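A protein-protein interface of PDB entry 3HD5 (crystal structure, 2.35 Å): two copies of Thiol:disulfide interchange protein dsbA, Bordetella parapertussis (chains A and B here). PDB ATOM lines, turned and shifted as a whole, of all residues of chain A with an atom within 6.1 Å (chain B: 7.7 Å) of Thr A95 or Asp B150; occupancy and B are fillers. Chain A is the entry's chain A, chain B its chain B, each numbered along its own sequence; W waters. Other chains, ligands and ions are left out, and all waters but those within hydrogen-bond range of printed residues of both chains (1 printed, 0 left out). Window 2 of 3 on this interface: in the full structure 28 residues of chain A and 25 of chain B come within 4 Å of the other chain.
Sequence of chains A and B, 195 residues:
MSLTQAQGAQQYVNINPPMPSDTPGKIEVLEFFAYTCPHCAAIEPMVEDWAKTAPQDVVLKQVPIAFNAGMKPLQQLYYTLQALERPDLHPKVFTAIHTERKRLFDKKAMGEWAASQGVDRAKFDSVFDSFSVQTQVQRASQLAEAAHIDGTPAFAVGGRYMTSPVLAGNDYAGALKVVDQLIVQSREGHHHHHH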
ATOM      1  N   ALA A  41      16.804   7.280  -4.147  1.00  0.00           N
ATOM      2  CA  ALA A  41      16.452   6.843  -2.797  1.00  0.00           C
ATOM      3  C   ALA A  41      15.708   5.524  -2.860  1.00  0.00           C
ATOM      4  O   ALA A  41      15.999   4.593  -2.107  1.00  0.00           O
ATOM      5  CB  ALA A  41      15.583   7.896  -2.101  1.00  0.00           C
ATOM      6  N   PRO A  45      18.210   0.492  -1.715  1.00  0.00           N
ATOM      7  CA  PRO A  45      18.226  -0.827  -1.078  1.00  0.00           C
ATOM      8  C   PRO A  45      18.312  -1.982  -2.075  1.00  0.00           C
ATOM      9  O   PRO A  45      18.806  -3.064  -1.742  1.00  0.00           O
ATOM     10  CB  PRO A  45      16.924  -0.848  -0.272  1.00  0.00           C
ATOM     11  CG  PRO A  45      16.048   0.138  -0.985  1.00  0.00           C
ATOM     12  CD  PRO A  45      16.998   1.242  -1.339  1.00  0.00           C
ATOM     13  N   PRO A  91      22.976   5.322   3.554  1.00  0.00           N
ATOM     14  CA  PRO A  91      21.581   5.096   3.153  1.00  0.00           C
ATOM     15  C   PRO A  91      20.576   5.909   3.967  1.00  0.00           C
ATOM     16  O   PRO A  91      19.493   6.255   3.482  1.00  0.00           O
ATOM     17  CB  PRO A  91      21.405   3.587   3.334  1.00  0.00           C
ATOM     18  CG  PRO A  91      22.396   3.250   4.418  1.00  0.00           C
ATOM     19  CD  PRO A  91      23.599   4.078   4.039  1.00  0.00           C
ATOM     20  N   LYS A  92      20.938   6.225   5.201  1.00  0.00           N
ATOM     21  CA  LYS A  92      20.054   6.994   6.060  1.00  0.00           C
ATOM     22  C   LYS A  92      19.835   8.409   5.532  1.00  0.00           C
ATOM     23  O   LYS A  92      18.796   9.016   5.801  1.00  0.00           O
ATOM     24  CB  LYS A  92      20.596   7.019   7.491  1.00  0.00           C
ATOM     25  CG  LYS A  92      20.519   5.657   8.185  1.00  0.00           C
ATOM     26  CD  LYS A  92      20.921   5.759   9.653  1.00  0.00           C
ATOM     27  CE  LYS A  92      20.898   4.398  10.355  1.00  0.00           C
ATOM     28  NZ  LYS A  92      19.538   3.787  10.408  1.00  0.00           N
ATOM     29  N   VAL A  93      20.801   8.928   4.774  1.00  0.00           N
ATOM     30  CA  VAL A  93      20.671  10.267   4.196  1.00  0.00           C
ATOM     31  C   VAL A  93      19.417  10.306   3.314  1.00  0.00           C
ATOM     32  O   VAL A  93      18.655  11.272   3.343  1.00  0.00           O
ATOM     33  CB  VAL A  93      21.898  10.634   3.308  1.00  0.00           C
ATOM     34  CG1 VAL A  93      21.654  11.963   2.585  1.00  0.00           C
ATOM     35  CG2 VAL A  93      23.146  10.724   4.157  1.00  0.00           C
ATOM     36  N   PHE A  94      19.216   9.258   2.520  1.00  0.00           N
ATOM     37  CA  PHE A  94      18.054   9.186   1.640  1.00  0.00           C
ATOM     38  C   PHE A  94      16.789   9.225   2.475  1.00  0.00           C
ATOM     39  O   PHE A  94      15.843   9.949   2.168  1.00  0.00           O
ATOM     40  CB  PHE A  94      18.064   7.887   0.825  1.00  0.00           C
ATOM     41  CG  PHE A  94      19.071   7.867  -0.298  1.00  0.00           C
ATOM     42  CD1 PHE A  94      18.954   8.745  -1.377  1.00  0.00           C
ATOM     43  CD2 PHE A  94      20.102   6.929  -0.310  1.00  0.00           C
ATOM     44  CE1 PHE A  94      19.849   8.681  -2.460  1.00  0.00           C
ATOM     45  CE2 PHE A  94      20.995   6.861  -1.384  1.00  0.00           C
ATOM     46  CZ  PHE A  94      20.864   7.740  -2.461  1.00  0.00           C
ATOM     47  N   THR A  95      16.781   8.435   3.540  1.00  0.00           N
ATOM     48  CA  THR A  95      15.626   8.373   4.398  1.00  0.00           C
ATOM     49  C   THR A  95      15.324   9.727   5.024  1.00  0.00           C
ATOM     50  O   THR A  95      14.177  10.150   5.055  1.00  0.00           O
ATOM     51  CB  THR A  95      15.822   7.332   5.506  1.00  0.00           C
ATOM     52  OG1 THR A  95      16.065   6.048   4.916  1.00  0.00           O
ATOM     53  CG2 THR A  95      14.575   7.260   6.386  1.00  0.00           C
ATOM     54  N   ALA A  96      16.353  10.417   5.500  1.00  0.00           N
ATOM     55  CA  ALA A  96      16.147  11.715   6.133  1.00  0.00           C
ATOM     56  C   ALA A  96      15.508  12.754   5.202  1.00  0.00           C
ATOM     57  O   ALA A  96      14.569  13.459   5.588  1.00  0.00           O
ATOM     58  CB  ALA A  96      17.473  12.244   6.680  1.00  0.00           C
ATOM     59  N   ILE A  97      16.020  12.847   3.981  1.00  0.00           N
ATOM     60  CA  ILE A  97      15.514  13.806   3.006  1.00  0.00           C
ATOM     61  C   ILE A  97      14.133  13.459   2.467  1.00  0.00           C
ATOM     62  O   ILE A  97      13.237  14.298   2.448  1.00  0.00           O
ATOM     63  CB  ILE A  97      16.466  13.923   1.779  1.00  0.00           C
ATOM     64  CG1 ILE A  97      17.784  14.581   2.187  1.00  0.00           C
ATOM     65  CG2 ILE A  97      15.796  14.708   0.666  1.00  0.00           C
ATOM     66  CD1 ILE A  97      18.820  14.601   1.065  1.00  0.00           C
ATOM     67  N   HIS A  98      13.971  12.219   2.026  1.00  0.00           N
ATOM     68  CA  HIS A  98      12.724  11.784   1.422  1.00  0.00           C
ATOM     69  C   HIS A  98      11.582  11.294   2.323  1.00  0.00           C
ATOM     70  O   HIS A  98      10.412  11.381   1.939  1.00  0.00           O
ATOM     71  CB  HIS A  98      13.057  10.739   0.361  1.00  0.00           C
ATOM     72  CG  HIS A  98      13.947  11.266  -0.721  1.00  0.00           C
ATOM     73  ND1 HIS A  98      13.489  12.085  -1.729  1.00  0.00           N
ATOM     74  CD2 HIS A  98      15.284  11.145  -0.914  1.00  0.00           C
ATOM     75  CE1 HIS A  98      14.500  12.447  -2.498  1.00  0.00           C
ATOM     76  NE2 HIS A  98      15.600  11.891  -2.024  1.00  0.00           N
ATOM     77  N   THR A  99      11.898  10.800   3.514  1.00  0.00           N
ATOM     78  CA  THR A  99      10.849  10.321   4.400  1.00  0.00           C
ATOM     79  C   THR A  99      10.604  11.236   5.601  1.00  0.00           C
ATOM     80  O   THR A  99       9.460  11.428   6.009  1.00  0.00           O
ATOM     81  CB  THR A  99      11.165   8.917   4.888  1.00  0.00           C
ATOM     82  OG1 THR A  99      11.204   8.034   3.762  1.00  0.00           O
ATOM     83  CG2 THR A  99      10.100   8.439   5.870  1.00  0.00           C
ATOM     84  N   GLU A 100      11.680  11.799   6.146  1.00  0.00           N
ATOM     85  CA  GLU A 100      11.605  12.697   7.296  1.00  0.00           C
ATOM     86  C   GLU A 100      11.513  14.136   6.795  1.00  0.00           C
ATOM     87  O   GLU A 100      11.366  15.073   7.572  1.00  0.00           O
ATOM     88  CB  GLU A 100      12.860  12.533   8.163  1.00  0.00           C
ATOM     89  CG  GLU A 100      13.210  11.088   8.479  1.00  0.00           C
ATOM     90  CD  GLU A 100      14.475  10.938   9.324  1.00  0.00           C
ATOM     91  OE1 GLU A 100      14.508  11.438  10.468  1.00  0.00           O
ATOM     92  OE2 GLU A 100      15.440  10.305   8.843  1.00  0.00           O
ATOM     93  N   ARG A 101      11.605  14.292   5.480  1.00  0.00           N
ATOM     94  CA  ARG A 101      11.542  15.597   4.831  1.00  0.00           C
ATOM     95  C   ARG A 101      12.501  16.603   5.460  1.00  0.00           C
ATOM     96  O   ARG A 101      12.189  17.787   5.576  1.00  0.00           O
ATOM     97  CB  ARG A 101      10.112  16.144   4.874  1.00  0.00           C
ATOM     98  CG  ARG A 101       9.064  15.159   4.385  1.00  0.00           C
ATOM     99  CD  ARG A 101       9.404  14.595   3.003  1.00  0.00           C
ATOM    100  NE  ARG A 101       9.333  15.597   1.939  1.00  0.00           N
ATOM    101  CZ  ARG A 101       9.431  15.318   0.639  1.00  0.00           C
ATOM    102  NH1 ARG A 101       9.610  14.065   0.236  1.00  0.00           N
ATOM    103  NH2 ARG A 101       9.342  16.290  -0.261  1.00  0.00           N
ATOM    104  N   LYS A 102      13.666  16.128   5.879  1.00  0.00           N
ATOM    105  CA  LYS A 102      14.652  17.017   6.464  1.00  0.00           C
ATOM    106  C   LYS A 102      15.407  17.687   5.328  1.00  0.00           C
ATOM    107  O   LYS A 102      15.781  17.034   4.357  1.00  0.00           O
ATOM    108  CB  LYS A 102      15.594  16.234   7.374  1.00  0.00           C
ATOM    109  CG  LYS A 102      14.887  15.751   8.624  1.00  0.00           C
ATOM    110  CD  LYS A 102      15.820  15.073   9.603  1.00  0.00           C
ATOM    111  CE  LYS A 102      15.108  14.861  10.925  1.00  0.00           C
ATOM    112  NZ  LYS A 102      15.912  14.043  11.858  1.00  0.00           N
ATOM    113  N   VAL B  13      13.081  -6.348  -2.725  1.00  0.00           N
ATOM    114  CA  VAL B  13      14.459  -6.514  -2.284  1.00  0.00           C
ATOM    115  C   VAL B  13      14.522  -7.623  -1.247  1.00  0.00           C
ATOM    116  O   VAL B  13      13.580  -7.810  -0.479  1.00  0.00           O
ATOM    117  CB  VAL B  13      15.004  -5.207  -1.655  1.00  0.00           C
ATOM    118  CG1 VAL B  13      14.975  -4.085  -2.678  1.00  0.00           C
ATOM    119  CG2 VAL B  13      14.164  -4.816  -0.450  1.00  0.00           C
ATOM    120  N   PHE B  32       5.148  -1.709   7.765  1.00  0.00           N
ATOM    121  CA  PHE B  32       5.819  -0.705   8.588  1.00  0.00           C
ATOM    122  C   PHE B  32       5.165   0.613   8.219  1.00  0.00           C
ATOM    123  O   PHE B  32       5.098   0.974   7.051  1.00  0.00           O
ATOM    124  CB  PHE B  32       7.316  -0.679   8.271  1.00  0.00           C
ATOM    125  CG  PHE B  32       8.046  -1.882   8.786  1.00  0.00           C
ATOM    126  CD1 PHE B  32       8.491  -1.926  10.109  1.00  0.00           C
ATOM    127  CD2 PHE B  32       8.200  -3.009   7.985  1.00  0.00           C
ATOM    128  CE1 PHE B  32       9.069  -3.079  10.626  1.00  0.00           C
ATOM    129  CE2 PHE B  32       8.776  -4.164   8.492  1.00  0.00           C
ATOM    130  CZ  PHE B  32       9.212  -4.201   9.819  1.00  0.00           C
ATOM    131  N   ILE B  65       6.732   2.674  12.992  1.00  0.00           N
ATOM    132  CA  ILE B  65       8.176   2.850  12.928  1.00  0.00           C
ATOM    133  C   ILE B  65       8.593   4.243  13.361  1.00  0.00           C
ATOM    134  O   ILE B  65       7.792   5.166  13.351  1.00  0.00           O
ATOM    135  CB  ILE B  65       8.677   2.587  11.489  1.00  0.00           C
ATOM    136  CG1 ILE B  65      10.195   2.402  11.483  1.00  0.00           C
ATOM    137  CG2 ILE B  65       8.279   3.745  10.585  1.00  0.00           C
ATOM    138  CD1 ILE B  65      10.754   1.987  10.134  1.00  0.00           C
ATOM    139  N   PHE B  67      11.964   6.884  12.769  1.00  0.00           N
ATOM    140  CA  PHE B  67      13.291   7.135  12.200  1.00  0.00           C
ATOM    141  C   PHE B  67      14.091   8.090  13.081  1.00  0.00           C
ATOM    142  O   PHE B  67      15.318   8.153  13.006  1.00  0.00           O
ATOM    143  CB  PHE B  67      13.170   7.684  10.774  1.00  0.00           C
ATOM    144  CG  PHE B  67      12.635   6.679   9.793  1.00  0.00           C
ATOM    145  CD1 PHE B  67      13.298   5.469   9.600  1.00  0.00           C
ATOM    146  CD2 PHE B  67      11.445   6.912   9.108  1.00  0.00           C
ATOM    147  CE1 PHE B  67      12.784   4.506   8.747  1.00  0.00           C
ATOM    148  CE2 PHE B  67      10.919   5.947   8.245  1.00  0.00           C
ATOM    149  CZ  PHE B  67      11.587   4.743   8.065  1.00  0.00           C
ATOM    150  N   ALA B 144      12.088  -3.182  12.835  1.00  0.00           N
ATOM    151  CA  ALA B 144      12.425  -2.221  11.791  1.00  0.00           C
ATOM    152  C   ALA B 144      13.910  -2.306  11.443  1.00  0.00           C
ATOM    153  O   ALA B 144      14.288  -2.233  10.273  1.00  0.00           O
ATOM    154  CB  ALA B 144      12.073  -0.810  12.241  1.00  0.00           C
ATOM    155  N   ALA B 147      14.685  -5.629   9.505  1.00  0.00           N
ATOM    156  CA  ALA B 147      14.207  -5.608   8.129  1.00  0.00           C
ATOM    157  C   ALA B 147      14.853  -4.490   7.326  1.00  0.00           C
ATOM    158  O   ALA B 147      14.548  -4.315   6.149  1.00  0.00           O
ATOM    159  CB  ALA B 147      12.691  -5.452   8.103  1.00  0.00           C
ATOM    160  N   HIS B 148      15.724  -3.723   7.974  1.00  0.00           N
ATOM    161  CA  HIS B 148      16.411  -2.629   7.305  1.00  0.00           C
ATOM    162  C   HIS B 148      15.430  -1.682   6.607  1.00  0.00           C
ATOM    163  O   HIS B 148      15.682  -1.235   5.487  1.00  0.00           O
ATOM    164  CB  HIS B 148      17.389  -3.205   6.273  1.00  0.00           C
ATOM    165  CG  HIS B 148      18.268  -4.287   6.818  1.00  0.00           C
ATOM    166  ND1 HIS B 148      19.273  -4.042   7.733  1.00  0.00           N
ATOM    167  CD2 HIS B 148      18.266  -5.627   6.610  1.00  0.00           C
ATOM    168  CE1 HIS B 148      19.849  -5.184   8.065  1.00  0.00           C
ATOM    169  NE2 HIS B 148      19.256  -6.161   7.399  1.00  0.00           N
ATOM    170  N   ILE B 149      14.323  -1.357   7.269  1.00  0.00           N
ATOM    171  CA  ILE B 149      13.338  -0.470   6.662  1.00  0.00           C
ATOM    172  C   ILE B 149      13.888   0.933   6.447  1.00  0.00           C
ATOM    173  O   ILE B 149      14.465   1.517   7.353  1.00  0.00           O
ATOM    174  CB  ILE B 149      12.060  -0.392   7.507  1.00  0.00           C
ATOM    175  CG1 ILE B 149      11.543  -1.806   7.788  1.00  0.00           C
ATOM    176  CG2 ILE B 149      11.002   0.408   6.764  1.00  0.00           C
ATOM    177  CD1 ILE B 149      11.343  -2.652   6.533  1.00  0.00           C
ATOM    178  N   ASP B 150      13.695   1.468   5.240  1.00  0.00           N
ATOM    179  CA  ASP B 150      14.206   2.789   4.897  1.00  0.00           C
ATOM    180  C   ASP B 150      13.133   3.809   4.543  1.00  0.00           C
ATOM    181  O   ASP B 150      13.443   4.974   4.277  1.00  0.00           O
ATOM    182  CB  ASP B 150      15.185   2.683   3.724  1.00  0.00           C
ATOM    183  CG  ASP B 150      16.341   1.741   4.014  1.00  0.00           C
ATOM    184  OD1 ASP B 150      16.991   1.901   5.074  1.00  0.00           O
ATOM    185  OD2 ASP B 150      16.604   0.842   3.183  1.00  0.00           O
ATOM    186  N   GLY B 151      11.877   3.380   4.531  1.00  0.00           N
ATOM    187  CA  GLY B 151      10.797   4.294   4.198  1.00  0.00           C
ATOM    188  C   GLY B 151       9.447   3.699   4.554  1.00  0.00           C
ATOM    189  O   GLY B 151       9.375   2.557   5.013  1.00  0.00           O
ATOM    190  N   THR B 152       8.378   4.462   4.347  1.00  0.00           N
ATOM    191  CA  THR B 152       7.033   3.986   4.649  1.00  0.00           C
ATOM    192  C   THR B 152       6.033   4.421   3.584  1.00  0.00           C
ATOM    193  O   THR B 152       6.150   5.500   3.001  1.00  0.00           O
ATOM    194  CB  THR B 152       6.526   4.524   6.006  1.00  0.00           C
ATOM    195  OG1 THR B 152       6.640   5.956   6.023  1.00  0.00           O
ATOM    196  CG2 THR B 152       7.321   3.928   7.156  1.00  0.00           C
ATOM    197  N   ALA B 154       6.201   0.260   4.113  1.00  0.00           N
ATOM    198  CA  ALA B 154       7.032  -0.804   3.582  1.00  0.00           C
ATOM    199  C   ALA B 154       6.437  -2.140   3.988  1.00  0.00           C
ATOM    200  O   ALA B 154       5.947  -2.295   5.103  1.00  0.00           O
ATOM    201  CB  ALA B 154       8.452  -0.676   4.107  1.00  0.00           C
ATOM    202  N   MET B 162      10.963  -7.602   0.815  1.00  0.00           N
ATOM    203  CA  MET B 162      10.494  -6.260   1.112  1.00  0.00           C
ATOM    204  C   MET B 162      10.106  -5.564  -0.190  1.00  0.00           C
ATOM    205  O   MET B 162      10.872  -5.554  -1.154  1.00  0.00           O
ATOM    206  CB  MET B 162      11.593  -5.468   1.837  1.00  0.00           C
ATOM    207  CG  MET B 162      11.169  -4.102   2.379  1.00  0.00           C
ATOM    208  SD  MET B 162      11.029  -2.675   1.032  1.00  0.00           S
ATOM    209  CE  MET B 162      12.845  -1.966   1.170  1.00  0.00           C
HETATM  210  O   HOH W   1      17.660   4.165   6.107  1.00  0.00           O
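Water W1 bridges the side-chain carboxylate (OD1) of Asp B150 and the side-chain hydroxyl (OG1) of Thr A95.
OG1 of Thr A95 lies within hydrogen-bond range of O of Asp B150 (2.9 Å).
The backbone NH (N) of Glu A100 lies within hydrogen-bond range of the backbone carbonyl oxygen (O) of Thr A95 (3.2 Å).
The backbone NH (N) of Ala A96 sits close to the side-chain carboxylate (OE2) of Glu A100 (3.5 Å).
The side-chain carboxylate (OE1) of Glu A100 is in salt-bridge range of the side-chain amino group (NZ) of Lys A102 (3.3 Å).
O of Met B162 is in hydrogen-bond range of N of Val B13.
Of the 14 printed residues of chain A, 4 touch a printed residue of chain B.
Printed residues of chain A that touch a printed residue of chain B: Pro A45, Thr A95, Thr A99 and Glu A100.
Along chain A the printed residues that touch a printed residue of chain B span positions 45 to 100.
Of chain A, only Pro A45, Thr A95 and Thr A99 come within 4 Å of Asp B150.
Of the printed residues of chain B, Thr A99 touches Phe B67, Asp B150 and Gly B151.
Printed residues of chain A within 4 Å of Val B13: Pro A45 (3.99 Å).
Printed residues of chain A within 4 Å of Phe B67: Thr A95 (3.9 Å), Thr A99 (3.5 Å) and Glu A100 (3.8 Å).
Arg A101 touches none of the printed residues of chain B.
The nearest residue of chain B that does not touch Thr A95 is Gly B151 (5.0 Å).
The nearest residue of chain A that does not touch Asp B150 is Pro A91 (5.0 Å).
No position is printed for both chains.
Of the 8 pairs that touch across the chains among the printed residues, none has its exchanged pair printed and touching as well.
Among the printed residues, pairs that only touch across the chains: Thr A99 with Phe B67, Thr A99 with Gly B151, Glu A100 with Phe B67, Thr A99 with Asp B150, Pro A45 with Asp B150, Thr A95 with Phe B67 and Pro A45 with Val B13.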
